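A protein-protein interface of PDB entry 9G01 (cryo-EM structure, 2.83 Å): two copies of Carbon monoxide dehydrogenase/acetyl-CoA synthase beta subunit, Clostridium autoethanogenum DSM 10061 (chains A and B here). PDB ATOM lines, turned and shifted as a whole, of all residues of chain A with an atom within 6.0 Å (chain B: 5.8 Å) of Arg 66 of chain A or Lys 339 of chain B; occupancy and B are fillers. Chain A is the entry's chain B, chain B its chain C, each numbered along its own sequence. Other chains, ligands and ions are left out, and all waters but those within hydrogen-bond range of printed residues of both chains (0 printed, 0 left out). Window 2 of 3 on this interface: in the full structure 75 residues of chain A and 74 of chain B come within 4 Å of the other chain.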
ATOM      1  N   CYS A  54      29.330   7.508  29.897  1.00  0.00           N
ATOM      2  CA  CYS A  54      28.620   8.705  29.463  1.00  0.00           C
ATOM      3  C   CYS A  54      28.190   9.507  30.680  1.00  0.00           C
ATOM      4  O   CYS A  54      27.690   8.945  31.663  1.00  0.00           O
ATOM      5  CB  CYS A  54      27.371   8.384  28.618  1.00  0.00           C
ATOM      6  SG  CYS A  54      27.676   7.585  27.018  1.00  0.00           S
ATOM      7  N   ARG A  55      28.413  10.810  30.625  1.00  0.00           N
ATOM      8  CA  ARG A  55      27.910  11.732  31.624  1.00  0.00           C
ATOM      9  C   ARG A  55      27.157  12.837  30.904  1.00  0.00           C
ATOM     10  O   ARG A  55      27.647  13.402  29.920  1.00  0.00           O
ATOM     11  CB  ARG A  55      29.021  12.284  32.520  1.00  0.00           C
ATOM     12  CG  ARG A  55      30.264  12.706  31.789  1.00  0.00           C
ATOM     13  CD  ARG A  55      31.406  12.886  32.789  1.00  0.00           C
ATOM     14  NE  ARG A  55      32.611  13.302  32.088  1.00  0.00           N
ATOM     15  CZ  ARG A  55      33.830  13.342  32.606  1.00  0.00           C
ATOM     16  NH1 ARG A  55      34.067  12.973  33.852  1.00  0.00           N
ATOM     17  NH2 ARG A  55      34.842  13.758  31.847  1.00  0.00           N
ATOM     18  N   VAL A  56      25.945  13.087  31.364  1.00  0.00           N
ATOM     19  CA  VAL A  56      25.099  14.135  30.838  1.00  0.00           C
ATOM     20  C   VAL A  56      24.939  15.186  31.929  1.00  0.00           C
ATOM     21  O   VAL A  56      25.174  14.936  33.114  1.00  0.00           O
ATOM     22  CB  VAL A  56      23.743  13.578  30.361  1.00  0.00           C
ATOM     23  CG1 VAL A  56      23.971  12.579  29.180  1.00  0.00           C
ATOM     24  CG2 VAL A  56      22.984  12.916  31.534  1.00  0.00           C
ATOM     25  N   VAL A  64      25.980  18.625  27.679  1.00  0.00           N
ATOM     26  CA  VAL A  64      25.627  17.391  26.981  1.00  0.00           C
ATOM     27  C   VAL A  64      24.306  16.868  27.521  1.00  0.00           C
ATOM     28  O   VAL A  64      24.122  16.735  28.737  1.00  0.00           O
ATOM     29  CB  VAL A  64      26.749  16.351  27.135  1.00  0.00           C
ATOM     30  CG1 VAL A  64      26.387  15.025  26.431  1.00  0.00           C
ATOM     31  CG2 VAL A  64      28.062  16.914  26.596  1.00  0.00           C
ATOM     32  N   GLU A  65      23.374  16.567  26.618  1.00  0.00           N
ATOM     33  CA  GLU A  65      22.031  16.154  27.011  1.00  0.00           C
ATOM     34  C   GLU A  65      21.846  14.647  27.016  1.00  0.00           C
ATOM     35  O   GLU A  65      21.123  14.129  27.867  1.00  0.00           O
ATOM     36  CB  GLU A  65      20.983  16.770  26.071  1.00  0.00           C
ATOM     37  CG  GLU A  65      21.155  18.274  25.824  1.00  0.00           C
ATOM     38  CD  GLU A  65      20.930  19.101  27.087  1.00  0.00           C
ATOM     39  OE1 GLU A  65      21.752  19.003  28.021  1.00  0.00           O
ATOM     40  OE2 GLU A  65      19.924  19.838  27.152  1.00  0.00           O
ATOM     41  N   ARG A  66      22.461  13.921  26.083  1.00  0.00           N
ATOM     42  CA  ARG A  66      22.196  12.499  25.948  1.00  0.00           C
ATOM     43  C   ARG A  66      23.496  11.711  25.952  1.00  0.00           C
ATOM     44  O   ARG A  66      24.530  12.184  25.477  1.00  0.00           O
ATOM     45  CB  ARG A  66      21.416  12.181  24.653  1.00  0.00           C
ATOM     46  CG  ARG A  66      20.018  12.810  24.605  1.00  0.00           C
ATOM     47  CD  ARG A  66      19.379  12.650  23.209  1.00  0.00           C
ATOM     48  NE  ARG A  66      17.980  13.070  23.206  1.00  0.00           N
ATOM     49  CZ  ARG A  66      16.933  12.259  23.302  1.00  0.00           C
ATOM     50  NH1 ARG A  66      17.068  10.944  23.351  1.00  0.00           N
ATOM     51  NH2 ARG A  66      15.710  12.783  23.342  1.00  0.00           N
ATOM     52  N   GLY A  67      23.412  10.479  26.438  1.00  0.00           N
ATOM     53  CA  GLY A  67      24.495   9.541  26.284  1.00  0.00           C
ATOM     54  C   GLY A  67      24.659   9.170  24.821  1.00  0.00           C
ATOM     55  O   GLY A  67      23.914   9.608  23.939  1.00  0.00           O
ATOM     56  N   ILE A  68      25.665   8.332  24.558  1.00  0.00           N
ATOM     57  CA  ILE A  68      26.009   7.977  23.184  1.00  0.00           C
ATOM     58  C   ILE A  68      24.867   7.233  22.499  1.00  0.00           C
ATOM     59  O   ILE A  68      24.563   7.474  21.327  1.00  0.00           O
ATOM     60  CB  ILE A  68      27.329   7.188  23.153  1.00  0.00           C
ATOM     61  CG1 ILE A  68      28.463   8.115  23.639  1.00  0.00           C
ATOM     62  CG2 ILE A  68      27.592   6.634  21.732  1.00  0.00           C
ATOM     63  CD1 ILE A  68      29.793   7.412  23.914  1.00  0.00           C
ATOM     64  N   GLY A  70      21.845   7.734  23.093  1.00  0.00           N
ATOM     65  CA  GLY A  70      20.716   8.639  23.090  1.00  0.00           C
ATOM     66  C   GLY A  70      19.915   8.705  24.380  1.00  0.00           C
ATOM     67  O   GLY A  70      18.902   9.408  24.419  1.00  0.00           O
ATOM     68  N   ALA A  71      20.345   8.023  25.440  1.00  0.00           N
ATOM     69  CA  ALA A  71      19.614   8.024  26.703  1.00  0.00           C
ATOM     70  C   ALA A  71      19.671   9.389  27.395  1.00  0.00           C
ATOM     71  O   ALA A  71      20.742   9.992  27.517  1.00  0.00           O
ATOM     72  CB  ALA A  71      20.184   6.937  27.619  1.00  0.00           C
ATOM     73  N   THR A  72      18.515   9.875  27.864  1.00  0.00           N
ATOM     74  CA  THR A  72      18.433  11.162  28.541  1.00  0.00           C
ATOM     75  C   THR A  72      18.898  11.060  29.993  1.00  0.00           C
ATOM     76  O   THR A  72      19.141   9.978  30.532  1.00  0.00           O
ATOM     77  CB  THR A  72      17.002  11.717  28.524  1.00  0.00           C
ATOM     78  OG1 THR A  72      16.110  10.794  29.167  1.00  0.00           O
ATOM     79  CG2 THR A  72      16.542  11.990  27.093  1.00  0.00           C
ATOM     80  N   ALA A  73      18.983  12.223  30.640  1.00  0.00           N
ATOM     81  CA  ALA A  73      19.334  12.236  32.053  1.00  0.00           C
ATOM     82  C   ALA A  73      18.300  11.465  32.863  1.00  0.00           C
ATOM     83  O   ALA A  73      18.662  10.647  33.710  1.00  0.00           O
ATOM     84  CB  ALA A  73      19.482  13.678  32.554  1.00  0.00           C
ATOM     85  N   ILE A  76      18.995   7.735  32.452  1.00  0.00           N
ATOM     86  CA  ILE A  76      20.201   7.306  33.169  1.00  0.00           C
ATOM     87  C   ILE A  76      19.934   7.253  34.666  1.00  0.00           C
ATOM     88  O   ILE A  76      20.300   6.284  35.350  1.00  0.00           O
ATOM     89  CB  ILE A  76      21.381   8.235  32.803  1.00  0.00           C
ATOM     90  CG1 ILE A  76      21.675   8.099  31.290  1.00  0.00           C
ATOM     91  CG2 ILE A  76      22.646   7.931  33.666  1.00  0.00           C
ATOM     92  CD1 ILE A  76      22.633   9.131  30.708  1.00  0.00           C
ATOM     93  N   GLU B  24      21.202  14.172  14.295  1.00  0.00           N
ATOM     94  CA  GLU B  24      22.417  13.673  14.916  1.00  0.00           C
ATOM     95  C   GLU B  24      22.376  12.155  15.021  1.00  0.00           C
ATOM     96  O   GLU B  24      21.318  11.556  15.229  1.00  0.00           O
ATOM     97  CB  GLU B  24      22.625  14.290  16.307  1.00  0.00           C
ATOM     98  CG  GLU B  24      21.715  13.693  17.379  1.00  0.00           C
ATOM     99  CD  GLU B  24      22.072  14.144  18.787  1.00  0.00           C
ATOM    100  OE1 GLU B  24      22.844  15.113  18.937  1.00  0.00           O
ATOM    101  OE2 GLU B  24      21.577  13.521  19.749  1.00  0.00           O
ATOM    102  N   ARG B  29      26.888  11.935  18.799  1.00  0.00           N
ATOM    103  CA  ARG B  29      26.830  11.908  20.260  1.00  0.00           C
ATOM    104  C   ARG B  29      28.156  11.441  20.852  1.00  0.00           C
ATOM    105  O   ARG B  29      28.621  11.997  21.854  1.00  0.00           O
ATOM    106  CB  ARG B  29      25.662  11.029  20.741  1.00  0.00           C
ATOM    107  CG  ARG B  29      24.276  11.634  20.396  1.00  0.00           C
ATOM    108  CD  ARG B  29      23.074  10.904  21.058  1.00  0.00           C
ATOM    109  NE  ARG B  29      22.972   9.494  20.681  1.00  0.00           N
ATOM    110  CZ  ARG B  29      22.487   9.039  19.530  1.00  0.00           C
ATOM    111  NH1 ARG B  29      22.048   9.856  18.586  1.00  0.00           N
ATOM    112  NH2 ARG B  29      22.451   7.723  19.315  1.00  0.00           N
ATOM    113  N   MET B  33      30.453  13.585  23.453  1.00  0.00           N
ATOM    114  CA  MET B  33      30.944  13.108  24.738  1.00  0.00           C
ATOM    115  C   MET B  33      32.414  13.450  24.955  1.00  0.00           C
ATOM    116  O   MET B  33      32.861  13.474  26.107  1.00  0.00           O
ATOM    117  CB  MET B  33      30.715  11.595  24.837  1.00  0.00           C
ATOM    118  CG  MET B  33      30.673  11.072  26.272  1.00  0.00           C
ATOM    119  SD  MET B  33      29.421  11.903  27.299  1.00  0.00           S
ATOM    120  CE  MET B  33      27.865  11.372  26.573  1.00  0.00           C
ATOM    121  N   PRO B 335      17.590   4.529  22.208  1.00  0.00           N
ATOM    122  CA  PRO B 335      16.431   5.393  22.509  1.00  0.00           C
ATOM    123  C   PRO B 335      16.383   6.623  21.627  1.00  0.00           C
ATOM    124  O   PRO B 335      15.291   7.138  21.366  1.00  0.00           O
ATOM    125  CB  PRO B 335      16.596   5.728  24.005  1.00  0.00           C
ATOM    126  CG  PRO B 335      18.037   5.421  24.347  1.00  0.00           C
ATOM    127  CD  PRO B 335      18.439   4.293  23.395  1.00  0.00           C
ATOM    128  N   ALA B 336      17.528   7.083  21.118  1.00  0.00           N
ATOM    129  CA  ALA B 336      17.528   8.249  20.243  1.00  0.00           C
ATOM    130  C   ALA B 336      16.619   8.056  19.039  1.00  0.00           C
ATOM    131  O   ALA B 336      16.184   9.049  18.449  1.00  0.00           O
ATOM    132  CB  ALA B 336      18.951   8.562  19.746  1.00  0.00           C
ATOM    133  N   LEU B 337      16.342   6.806  18.654  1.00  0.00           N
ATOM    134  CA  LEU B 337      15.417   6.562  17.551  1.00  0.00           C
ATOM    135  C   LEU B 337      14.123   7.343  17.716  1.00  0.00           C
ATOM    136  O   LEU B 337      13.586   7.862  16.742  1.00  0.00           O
ATOM    137  CB  LEU B 337      15.097   5.065  17.434  1.00  0.00           C
ATOM    138  CG  LEU B 337      16.185   4.180  16.802  1.00  0.00           C
ATOM    139  CD1 LEU B 337      15.835   2.688  16.955  1.00  0.00           C
ATOM    140  CD2 LEU B 337      16.438   4.554  15.320  1.00  0.00           C
ATOM    141  N   ALA B 338      13.565   7.379  18.928  1.00  0.00           N
ATOM    142  CA  ALA B 338      12.324   8.123  19.124  1.00  0.00           C
ATOM    143  C   ALA B 338      12.461   9.566  18.654  1.00  0.00           C
ATOM    144  O   ALA B 338      11.686  10.041  17.819  1.00  0.00           O
ATOM    145  CB  ALA B 338      11.906   8.067  20.595  1.00  0.00           C
ATOM    146  N   LYS B 339      13.485  10.266  19.148  1.00  0.00           N
ATOM    147  CA  LYS B 339      13.727  11.632  18.698  1.00  0.00           C
ATOM    148  C   LYS B 339      13.909  11.684  17.184  1.00  0.00           C
ATOM    149  O   LYS B 339      13.272  12.489  16.498  1.00  0.00           O
ATOM    150  CB  LYS B 339      14.942  12.215  19.426  1.00  0.00           C
ATOM    151  CG  LYS B 339      15.236  13.672  19.052  1.00  0.00           C
ATOM    152  CD  LYS B 339      16.455  14.224  19.821  1.00  0.00           C
ATOM    153  CE  LYS B 339      16.725  15.685  19.424  1.00  0.00           C
ATOM    154  NZ  LYS B 339      17.888  16.271  20.180  1.00  0.00           N
ATOM    155  N   LEU B 340      14.713  10.767  16.642  1.00  0.00           N
ATOM    156  CA  LEU B 340      14.979  10.756  15.206  1.00  0.00           C
ATOM    157  C   LEU B 340      13.698  10.572  14.398  1.00  0.00           C
ATOM    158  O   LEU B 340      13.516  11.220  13.361  1.00  0.00           O
ATOM    159  CB  LEU B 340      16.012   9.665  14.881  1.00  0.00           C
ATOM    160  CG  LEU B 340      16.462   9.526  13.416  1.00  0.00           C
ATOM    161  CD1 LEU B 340      17.205  10.798  12.936  1.00  0.00           C
ATOM    162  CD2 LEU B 340      17.322   8.260  13.211  1.00  0.00           C
ATOM    163  N   SER B 341      12.759   9.765  14.899  1.00  0.00           N
ATOM    164  CA  SER B 341      11.517   9.479  14.183  1.00  0.00           C
ATOM    165  C   SER B 341      10.649  10.712  14.005  1.00  0.00           C
ATOM    166  O   SER B 341       9.810  10.739  13.102  1.00  0.00           O
ATOM    167  CB  SER B 341      10.709   8.383  14.895  1.00  0.00           C
ATOM    168  OG  SER B 341      11.260   7.111  14.596  1.00  0.00           O
ATOM    169  N   LYS B 342      10.875  11.755  14.802  1.00  0.00           N
ATOM    170  CA  LYS B 342      10.117  12.993  14.647  1.00  0.00           C
ATOM    171  C   LYS B 342      10.517  13.731  13.379  1.00  0.00           C
ATOM    172  O   LYS B 342       9.704  14.464  12.809  1.00  0.00           O
ATOM    173  CB  LYS B 342      10.312  13.903  15.864  1.00  0.00           C
ATOM    174  CG  LYS B 342      10.177  13.173  17.203  1.00  0.00           C
ATOM    175  CD  LYS B 342       8.793  12.512  17.349  1.00  0.00           C
ATOM    176  CE  LYS B 342       8.819  11.435  18.451  1.00  0.00           C
ATOM    177  NZ  LYS B 342       9.527  11.941  19.686  1.00  0.00           N
ATOM    178  N   SER B 343      11.750  13.534  12.909  1.00  0.00           N
ATOM    179  CA  SER B 343      12.229  14.224  11.719  1.00  0.00           C
ATOM    180  C   SER B 343      11.743  13.565  10.433  1.00  0.00           C
ATOM    181  O   SER B 343      12.011  14.092   9.349  1.00  0.00           O
ATOM    182  CB  SER B 343      13.769  14.293  11.709  1.00  0.00           C
ATOM    183  OG  SER B 343      14.267  15.141  12.739  1.00  0.00           O
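Hydrophobic or aromatic side chains of chain A that line the printed part of chain B: Val 64.
Along chain A the printed residues that touch a printed residue of chain B span positions 54 to 71.
Of the 12 printed residues of chain B, 5 touch a printed residue of chain A.
Printed residues of chain B that touch a printed residue of chain A: Arg 29, Met 33, Pro 335, Ala 336 and Lys 339.
Hydrophobic or aromatic side chains of chain B within 4 Å of the printed part of chain A: Met 33, Pro 335 and Ala 336.
Among the printed residues, 12 pairs touch across the chains.
The side-chain sulfur (SG) of Cys 54 of chain A sits close to the backbone NH (N) of Ile 68 of chain A, 3.3 Å away.
The backbone carbonyl oxygen (O) of Gly 70 of chain A is in hydrogen-bond range of the guanidinium group (NH1) of Arg 66 of chain A.
The side-chain carboxylate (OE2) of Glu 24 of chain B lies within salt-bridge range of the guanidinium group (NH1) of Arg 29 of chain B (3.9 Å).
Among the printed residues, merely in contact across the chains: Arg 66 of chain A with Met 33 of chain B, Ala 71 of chain A with Pro 335 of chain B, Cys 54 of chain A with Met 33 of chain B, Gly 70 of chain A with Ala 336 of chain B, Gly 70 of chain A with Pro 335 of chain B, Gly 67 of chain A with Met 33 of chain B, Arg 66 of chain A with Lys 339 of chain B and Val 64 of chain A with Met 33 of chain B.
No position is printed for both chains.
Lys 339 of chain B touches one residue of chain A.
Printed residues of chain B within 4 Å of Ile 68 of chain A: Arg 29.
Of the printed residues of chain B, Ala 71 of chain A touches Pro 335.
The nearest printed residue of chain B that does not touch Arg 66 of chain A is Ala 336 of chain B (4.1 Å).
The side-chain sulfur (SD) of Met 33 of chain B lies within hydrogen-bond range of the backbone NH (N) of Arg 55 of chain A (3.6 Å).
The backbone carbonyl oxygen of Gly 67 of chain A sits close to the guanidinium group of Arg 29 of chain B, at 3.4 Å.
NE of Arg 29 of chain B sits at hydrogen-bond distance from O of Ile 68 of chain A, 2.7 Å away.
NE of Arg 29 of chain B sits close to N of Gly 70 of chain A.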
